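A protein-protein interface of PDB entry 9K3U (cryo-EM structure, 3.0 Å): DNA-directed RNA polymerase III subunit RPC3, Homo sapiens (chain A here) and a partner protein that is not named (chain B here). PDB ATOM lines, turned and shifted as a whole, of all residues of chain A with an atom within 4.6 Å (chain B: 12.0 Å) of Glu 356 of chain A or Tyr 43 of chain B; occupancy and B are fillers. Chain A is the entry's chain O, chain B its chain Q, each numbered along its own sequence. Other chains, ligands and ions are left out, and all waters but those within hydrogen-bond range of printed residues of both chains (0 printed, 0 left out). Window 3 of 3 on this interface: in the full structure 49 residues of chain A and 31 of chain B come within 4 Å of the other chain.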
ATOM      1  N   SER A 352       3.066   9.040   0.653  1.00  0.00           N
ATOM      2  CA  SER A 352       2.700   7.822  -0.062  1.00  0.00           C
ATOM      3  C   SER A 352       3.885   6.868  -0.168  1.00  0.00           C
ATOM      4  O   SER A 352       3.736   5.657   0.039  1.00  0.00           O
ATOM      5  CB  SER A 352       2.169   8.171  -1.451  1.00  0.00           C
ATOM      6  OG  SER A 352       1.815   7.000  -2.170  1.00  0.00           O
ATOM      7  N   VAL A 353       5.071   7.392  -0.491  1.00  0.00           N
ATOM      8  CA  VAL A 353       6.238   6.520  -0.579  1.00  0.00           C
ATOM      9  C   VAL A 353       6.594   5.973   0.798  1.00  0.00           C
ATOM     10  O   VAL A 353       6.996   4.809   0.924  1.00  0.00           O
ATOM     11  CB  VAL A 353       7.421   7.257  -1.238  1.00  0.00           C
ATOM     12  CG1 VAL A 353       7.884   8.433  -0.394  1.00  0.00           C
ATOM     13  CG2 VAL A 353       8.575   6.291  -1.515  1.00  0.00           C
ATOM     14  N   VAL A 354       6.437   6.777   1.852  1.00  0.00           N
ATOM     15  CA  VAL A 354       6.687   6.274   3.200  1.00  0.00           C
ATOM     16  C   VAL A 354       5.722   5.141   3.530  1.00  0.00           C
ATOM     17  O   VAL A 354       6.116   4.112   4.091  1.00  0.00           O
ATOM     18  CB  VAL A 354       6.589   7.420   4.225  1.00  0.00           C
ATOM     19  CG1 VAL A 354       6.532   6.868   5.647  1.00  0.00           C
ATOM     20  CG2 VAL A 354       7.765   8.377   4.066  1.00  0.00           C
ATOM     21  N   GLN A 355       4.444   5.313   3.188  1.00  0.00           N
ATOM     22  CA  GLN A 355       3.457   4.272   3.457  1.00  0.00           C
ATOM     23  C   GLN A 355       3.784   2.994   2.696  1.00  0.00           C
ATOM     24  O   GLN A 355       3.696   1.891   3.249  1.00  0.00           O
ATOM     25  CB  GLN A 355       2.060   4.769   3.088  1.00  0.00           C
ATOM     26  CG  GLN A 355       0.940   3.795   3.424  1.00  0.00           C
ATOM     27  CD  GLN A 355      -0.430   4.336   3.061  1.00  0.00           C
ATOM     28  OE1 GLN A 355      -0.562   5.474   2.615  1.00  0.00           O
ATOM     29  NE2 GLN A 355      -1.458   3.515   3.252  1.00  0.00           N
ATOM     30  N   GLU A 356       4.161   3.121   1.423  1.00  0.00           N
ATOM     31  CA  GLU A 356       4.455   1.949   0.610  1.00  0.00           C
ATOM     32  C   GLU A 356       5.765   1.276   0.997  1.00  0.00           C
ATOM     33  O   GLU A 356       5.931   0.080   0.734  1.00  0.00           O
ATOM     34  CB  GLU A 356       4.502   2.334  -0.869  1.00  0.00           C
ATOM     35  CG  GLU A 356       3.176   2.836  -1.423  1.00  0.00           C
ATOM     36  CD  GLU A 356       2.109   1.761  -1.452  1.00  0.00           C
ATOM     37  OE1 GLU A 356       2.442   0.580  -1.216  1.00  0.00           O
ATOM     38  OE2 GLU A 356       0.931   2.098  -1.707  1.00  0.00           O
ATOM     39  N   ARG A 357       6.693   2.007   1.613  1.00  0.00           N
ATOM     40  CA  ARG A 357       7.991   1.449   1.973  1.00  0.00           C
ATOM     41  C   ARG A 357       8.053   0.919   3.398  1.00  0.00           C
ATOM     42  O   ARG A 357       8.871   0.038   3.677  1.00  0.00           O
ATOM     43  CB  ARG A 357       9.086   2.506   1.784  1.00  0.00           C
ATOM     44  CG  ARG A 357      10.500   1.981   1.978  1.00  0.00           C
ATOM     45  CD  ARG A 357      11.532   3.063   1.703  1.00  0.00           C
ATOM     46  NE  ARG A 357      12.898   2.573   1.855  1.00  0.00           N
ATOM     47  CZ  ARG A 357      13.984   3.329   1.736  1.00  0.00           C
ATOM     48  NH1 ARG A 357      13.872   4.622   1.462  1.00  0.00           N
ATOM     49  NH2 ARG A 357      15.187   2.793   1.891  1.00  0.00           N
ATOM     50  N   PHE A 358       7.216   1.429   4.307  1.00  0.00           N
ATOM     51  CA  PHE A 358       7.263   1.011   5.701  1.00  0.00           C
ATOM     52  C   PHE A 358       5.905   0.641   6.281  1.00  0.00           C
ATOM     53  O   PHE A 358       5.860   0.035   7.357  1.00  0.00           O
ATOM     54  CB  PHE A 358       7.891   2.116   6.564  1.00  0.00           C
ATOM     55  CG  PHE A 358       9.284   2.491   6.143  1.00  0.00           C
ATOM     56  CD1 PHE A 358      10.357   1.670   6.448  1.00  0.00           C
ATOM     57  CD2 PHE A 358       9.517   3.660   5.442  1.00  0.00           C
ATOM     58  CE1 PHE A 358      11.638   2.012   6.063  1.00  0.00           C
ATOM     59  CE2 PHE A 358      10.796   4.007   5.054  1.00  0.00           C
ATOM     60  CZ  PHE A 358      11.856   3.181   5.364  1.00  0.00           C
ATOM     61  N   GLY A 359       4.806   0.979   5.615  1.00  0.00           N
ATOM     62  CA  GLY A 359       3.485   0.570   6.055  1.00  0.00           C
ATOM     63  C   GLY A 359       2.651   1.732   6.563  1.00  0.00           C
ATOM     64  O   GLY A 359       3.110   2.868   6.724  1.00  0.00           O
ATOM     65  N   PHE B  38      20.644 -10.113   0.209  1.00  0.00           N
ATOM     66  CA  PHE B  38      19.392  -9.472  -0.192  1.00  0.00           C
ATOM     67  C   PHE B  38      18.324  -9.838   0.829  1.00  0.00           C
ATOM     68  O   PHE B  38      17.608 -10.836   0.660  1.00  0.00           O
ATOM     69  CB  PHE B  38      18.983  -9.899  -1.602  1.00  0.00           C
ATOM     70  CG  PHE B  38      19.958  -9.488  -2.667  1.00  0.00           C
ATOM     71  CD1 PHE B  38      19.875  -8.237  -3.257  1.00  0.00           C
ATOM     72  CD2 PHE B  38      20.959 -10.352  -3.078  1.00  0.00           C
ATOM     73  CE1 PHE B  38      20.770  -7.857  -4.238  1.00  0.00           C
ATOM     74  CE2 PHE B  38      21.858  -9.975  -4.059  1.00  0.00           C
ATOM     75  CZ  PHE B  38      21.764  -8.726  -4.639  1.00  0.00           C
ATOM     76  N   PRO B  39      18.185  -9.060   1.901  1.00  0.00           N
ATOM     77  CA  PRO B  39      17.193  -9.405   2.926  1.00  0.00           C
ATOM     78  C   PRO B  39      15.773  -9.255   2.406  1.00  0.00           C
ATOM     79  O   PRO B  39      15.454  -8.324   1.664  1.00  0.00           O
ATOM     80  CB  PRO B  39      17.488  -8.407   4.053  1.00  0.00           C
ATOM     81  CG  PRO B  39      18.134  -7.252   3.377  1.00  0.00           C
ATOM     82  CD  PRO B  39      18.923  -7.828   2.238  1.00  0.00           C
ATOM     83  N   ASP B  40      14.917 -10.191   2.803  1.00  0.00           N
ATOM     84  CA  ASP B  40      13.533 -10.181   2.357  1.00  0.00           C
ATOM     85  C   ASP B  40      12.762  -9.042   3.010  1.00  0.00           C
ATOM     86  O   ASP B  40      13.077  -8.598   4.119  1.00  0.00           O
ATOM     87  CB  ASP B  40      12.858 -11.517   2.675  1.00  0.00           C
ATOM     88  CG  ASP B  40      12.903 -11.852   4.155  1.00  0.00           C
ATOM     89  OD1 ASP B  40      13.545 -11.104   4.920  1.00  0.00           O
ATOM     90  OD2 ASP B  40      12.296 -12.872   4.550  1.00  0.00           O
ATOM     91  N   THR B  41      11.737  -8.563   2.305  1.00  0.00           N
ATOM     92  CA  THR B  41      10.886  -7.484   2.780  1.00  0.00           C
ATOM     93  C   THR B  41       9.427  -7.899   2.651  1.00  0.00           C
ATOM     94  O   THR B  41       9.033  -8.519   1.660  1.00  0.00           O
ATOM     95  CB  THR B  41      11.126  -6.187   1.996  1.00  0.00           C
ATOM     96  OG1 THR B  41      10.902  -6.420   0.598  1.00  0.00           O
ATOM     97  CG2 THR B  41      12.548  -5.693   2.205  1.00  0.00           C
ATOM     98  N   ASP B  42       8.628  -7.553   3.662  1.00  0.00           N
ATOM     99  CA  ASP B  42       7.212  -7.894   3.666  1.00  0.00           C
ATOM    100  C   ASP B  42       6.366  -6.947   2.827  1.00  0.00           C
ATOM    101  O   ASP B  42       5.173  -7.211   2.639  1.00  0.00           O
ATOM    102  CB  ASP B  42       6.680  -7.915   5.102  1.00  0.00           C
ATOM    103  CG  ASP B  42       6.925  -6.611   5.834  1.00  0.00           C
ATOM    104  OD1 ASP B  42       7.654  -5.754   5.294  1.00  0.00           O
ATOM    105  OD2 ASP B  42       6.389  -6.445   6.952  1.00  0.00           O
ATOM    106  N   TYR B  43       6.943  -5.859   2.320  1.00  0.00           N
ATOM    107  CA  TYR B  43       6.243  -4.916   1.458  1.00  0.00           C
ATOM    108  C   TYR B  43       6.731  -5.087   0.027  1.00  0.00           C
ATOM    109  O   TYR B  43       7.941  -5.081  -0.225  1.00  0.00           O
ATOM    110  CB  TYR B  43       6.465  -3.474   1.923  1.00  0.00           C
ATOM    111  CG  TYR B  43       5.871  -3.165   3.278  1.00  0.00           C
ATOM    112  CD1 TYR B  43       4.520  -2.883   3.418  1.00  0.00           C
ATOM    113  CD2 TYR B  43       6.667  -3.147   4.417  1.00  0.00           C
ATOM    114  CE1 TYR B  43       3.974  -2.598   4.656  1.00  0.00           C
ATOM    115  CE2 TYR B  43       6.129  -2.862   5.658  1.00  0.00           C
ATOM    116  CZ  TYR B  43       4.783  -2.589   5.772  1.00  0.00           C
ATOM    117  OH  TYR B  43       4.244  -2.303   7.006  1.00  0.00           O
ATOM    118  N   LYS B  44       5.789  -5.240  -0.907  1.00  0.00           N
ATOM    119  CA  LYS B  44       6.113  -5.419  -2.310  1.00  0.00           C
ATOM    120  C   LYS B  44       5.788  -4.153  -3.099  1.00  0.00           C
ATOM    121  O   LYS B  44       4.916  -3.374  -2.702  1.00  0.00           O
ATOM    122  CB  LYS B  44       5.337  -6.597  -2.913  1.00  0.00           C
ATOM    123  CG  LYS B  44       5.552  -7.927  -2.194  1.00  0.00           C
ATOM    124  CD  LYS B  44       7.015  -8.363  -2.194  1.00  0.00           C
ATOM    125  CE  LYS B  44       7.541  -8.594  -3.603  1.00  0.00           C
ATOM    126  NZ  LYS B  44       8.931  -9.128  -3.597  1.00  0.00           N
ATOM    127  N   PRO B  45       6.471  -3.914  -4.222  1.00  0.00           N
ATOM    128  CA  PRO B  45       6.166  -2.721  -5.019  1.00  0.00           C
ATOM    129  C   PRO B  45       4.731  -2.735  -5.521  1.00  0.00           C
ATOM    130  O   PRO B  45       4.174  -3.789  -5.841  1.00  0.00           O
ATOM    131  CB  PRO B  45       7.168  -2.799  -6.177  1.00  0.00           C
ATOM    132  CG  PRO B  45       8.256  -3.692  -5.693  1.00  0.00           C
ATOM    133  CD  PRO B  45       7.598  -4.678  -4.783  1.00  0.00           C
ATOM    134  N   VAL B  46       4.135  -1.555  -5.586  1.00  0.00           N
ATOM    135  CA  VAL B  46       2.764  -1.433  -6.102  1.00  0.00           C
ATOM    136  C   VAL B  46       2.774  -1.707  -7.602  1.00  0.00           C
ATOM    137  O   VAL B  46       3.679  -1.225  -8.306  1.00  0.00           O
ATOM    138  CB  VAL B  46       2.203  -0.041  -5.794  1.00  0.00           C
ATOM    139  CG1 VAL B  46       0.755   0.085  -6.257  1.00  0.00           C
ATOM    140  CG2 VAL B  46       2.316   0.258  -4.306  1.00  0.00           C
ATOM    141  N   PRO B  47       1.814  -2.463  -8.137  1.00  0.00           N
ATOM    142  CA  PRO B  47       1.836  -2.755  -9.576  1.00  0.00           C
ATOM    143  C   PRO B  47       1.743  -1.488 -10.412  1.00  0.00           C
ATOM    144  O   PRO B  47       1.277  -0.444  -9.953  1.00  0.00           O
ATOM    145  CB  PRO B  47       0.610  -3.655  -9.777  1.00  0.00           C
ATOM    146  CG  PRO B  47      -0.269  -3.382  -8.603  1.00  0.00           C
ATOM    147  CD  PRO B  47       0.661  -3.089  -7.469  1.00  0.00           C
ATOM    148  N   LEU B  48       2.196  -1.597 -11.659  1.00  0.00           N
ATOM    149  CA  LEU B  48       2.214  -0.452 -12.553  1.00  0.00           C
ATOM    150  C   LEU B  48       0.796  -0.059 -12.959  1.00  0.00           C
ATOM    151  O   LEU B  48      -0.114  -0.889 -13.037  1.00  0.00           O
ATOM    152  CB  LEU B  48       3.044  -0.757 -13.802  1.00  0.00           C
ATOM    153  CG  LEU B  48       4.556  -0.934 -13.628  1.00  0.00           C
ATOM    154  CD1 LEU B  48       5.169   0.271 -12.924  1.00  0.00           C
ATOM    155  CD2 LEU B  48       4.882  -2.218 -12.880  1.00  0.00           C
ATOM    156  N   LYS B  49       0.619   1.232 -13.220  1.00  0.00           N
ATOM    157  CA  LYS B  49      -0.661   1.729 -13.702  1.00  0.00           C
ATOM    158  C   LYS B  49      -0.960   1.156 -15.080  1.00  0.00           C
ATOM    159  O   LYS B  49      -0.108   1.160 -15.971  1.00  0.00           O
ATOM    160  CB  LYS B  49      -0.651   3.257 -13.758  1.00  0.00           C
ATOM    161  CG  LYS B  49      -0.401   3.929 -12.414  1.00  0.00           C
ATOM    162  CD  LYS B  49      -0.247   5.439 -12.551  1.00  0.00           C
ATOM    163  CE  LYS B  49      -1.525   6.107 -13.045  1.00  0.00           C
ATOM    164  NZ  LYS B  49      -2.682   5.851 -12.146  1.00  0.00           N
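The backbone carbonyl oxygen (O) of Phe 358 of chain A sits at hydrogen-bond distance from the side-chain hydroxyl (OH) of Tyr 43 of chain B.
The side-chain hydroxyl (OG1) of Thr 41 of chain B sits at hydrogen-bond distance from the backbone carbonyl oxygen (O) of Tyr 43 of chain B, 3.4 Å away.
Among the printed residues, pairs that only touch across the chains: Glu 356 of chain A with Tyr 43 of chain B (3.8 Å), Glu 356 of chain A with Val 46 of chain B (3.1 Å), Arg 357 of chain A with Tyr 43 of chain B (3.9 Å) and Gly 359 of chain A with Tyr 43 of chain B (3.1 Å).
Glu 356 of chain A touches two residues of chain B. Tyr 43 of chain B touches just these residues of chain A: Glu 356 (3.8 Å), Arg 357 (3.9 Å), Phe 358 (2.9 Å) and Gly 359 (3.1 Å). No residue of chain B comes within 4 Å of Ser 352 of chain A. Val 353 of chain A touches none of the printed residues of chain B. Phe 358 of chain A touches one residue of chain B. Gly 359 of chain A touches one residue of chain B. Of the printed residues of chain B, Arg 357 of chain A touches Tyr 43 (3.9 Å). Of the printed residues of chain A, Val 46 of chain B touches Glu 356. Lys 49 of chain B touches none of the printed residues of chain A. Phe 38 of chain B touches none of the printed residues of chain A. The nearest residue of chain B that does not touch Glu 356 of chain A is Lys 44 of chain B (4.9 Å). The nearest printed residue of chain A that does not touch Tyr 43 of chain B is Gln 355 of chain A (4.7 Å).
Of the 12 printed residues of chain B, 2 touch a printed residue of chain A. Along chain B the printed residues that touch a printed residue of chain A span positions 43 to 46.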
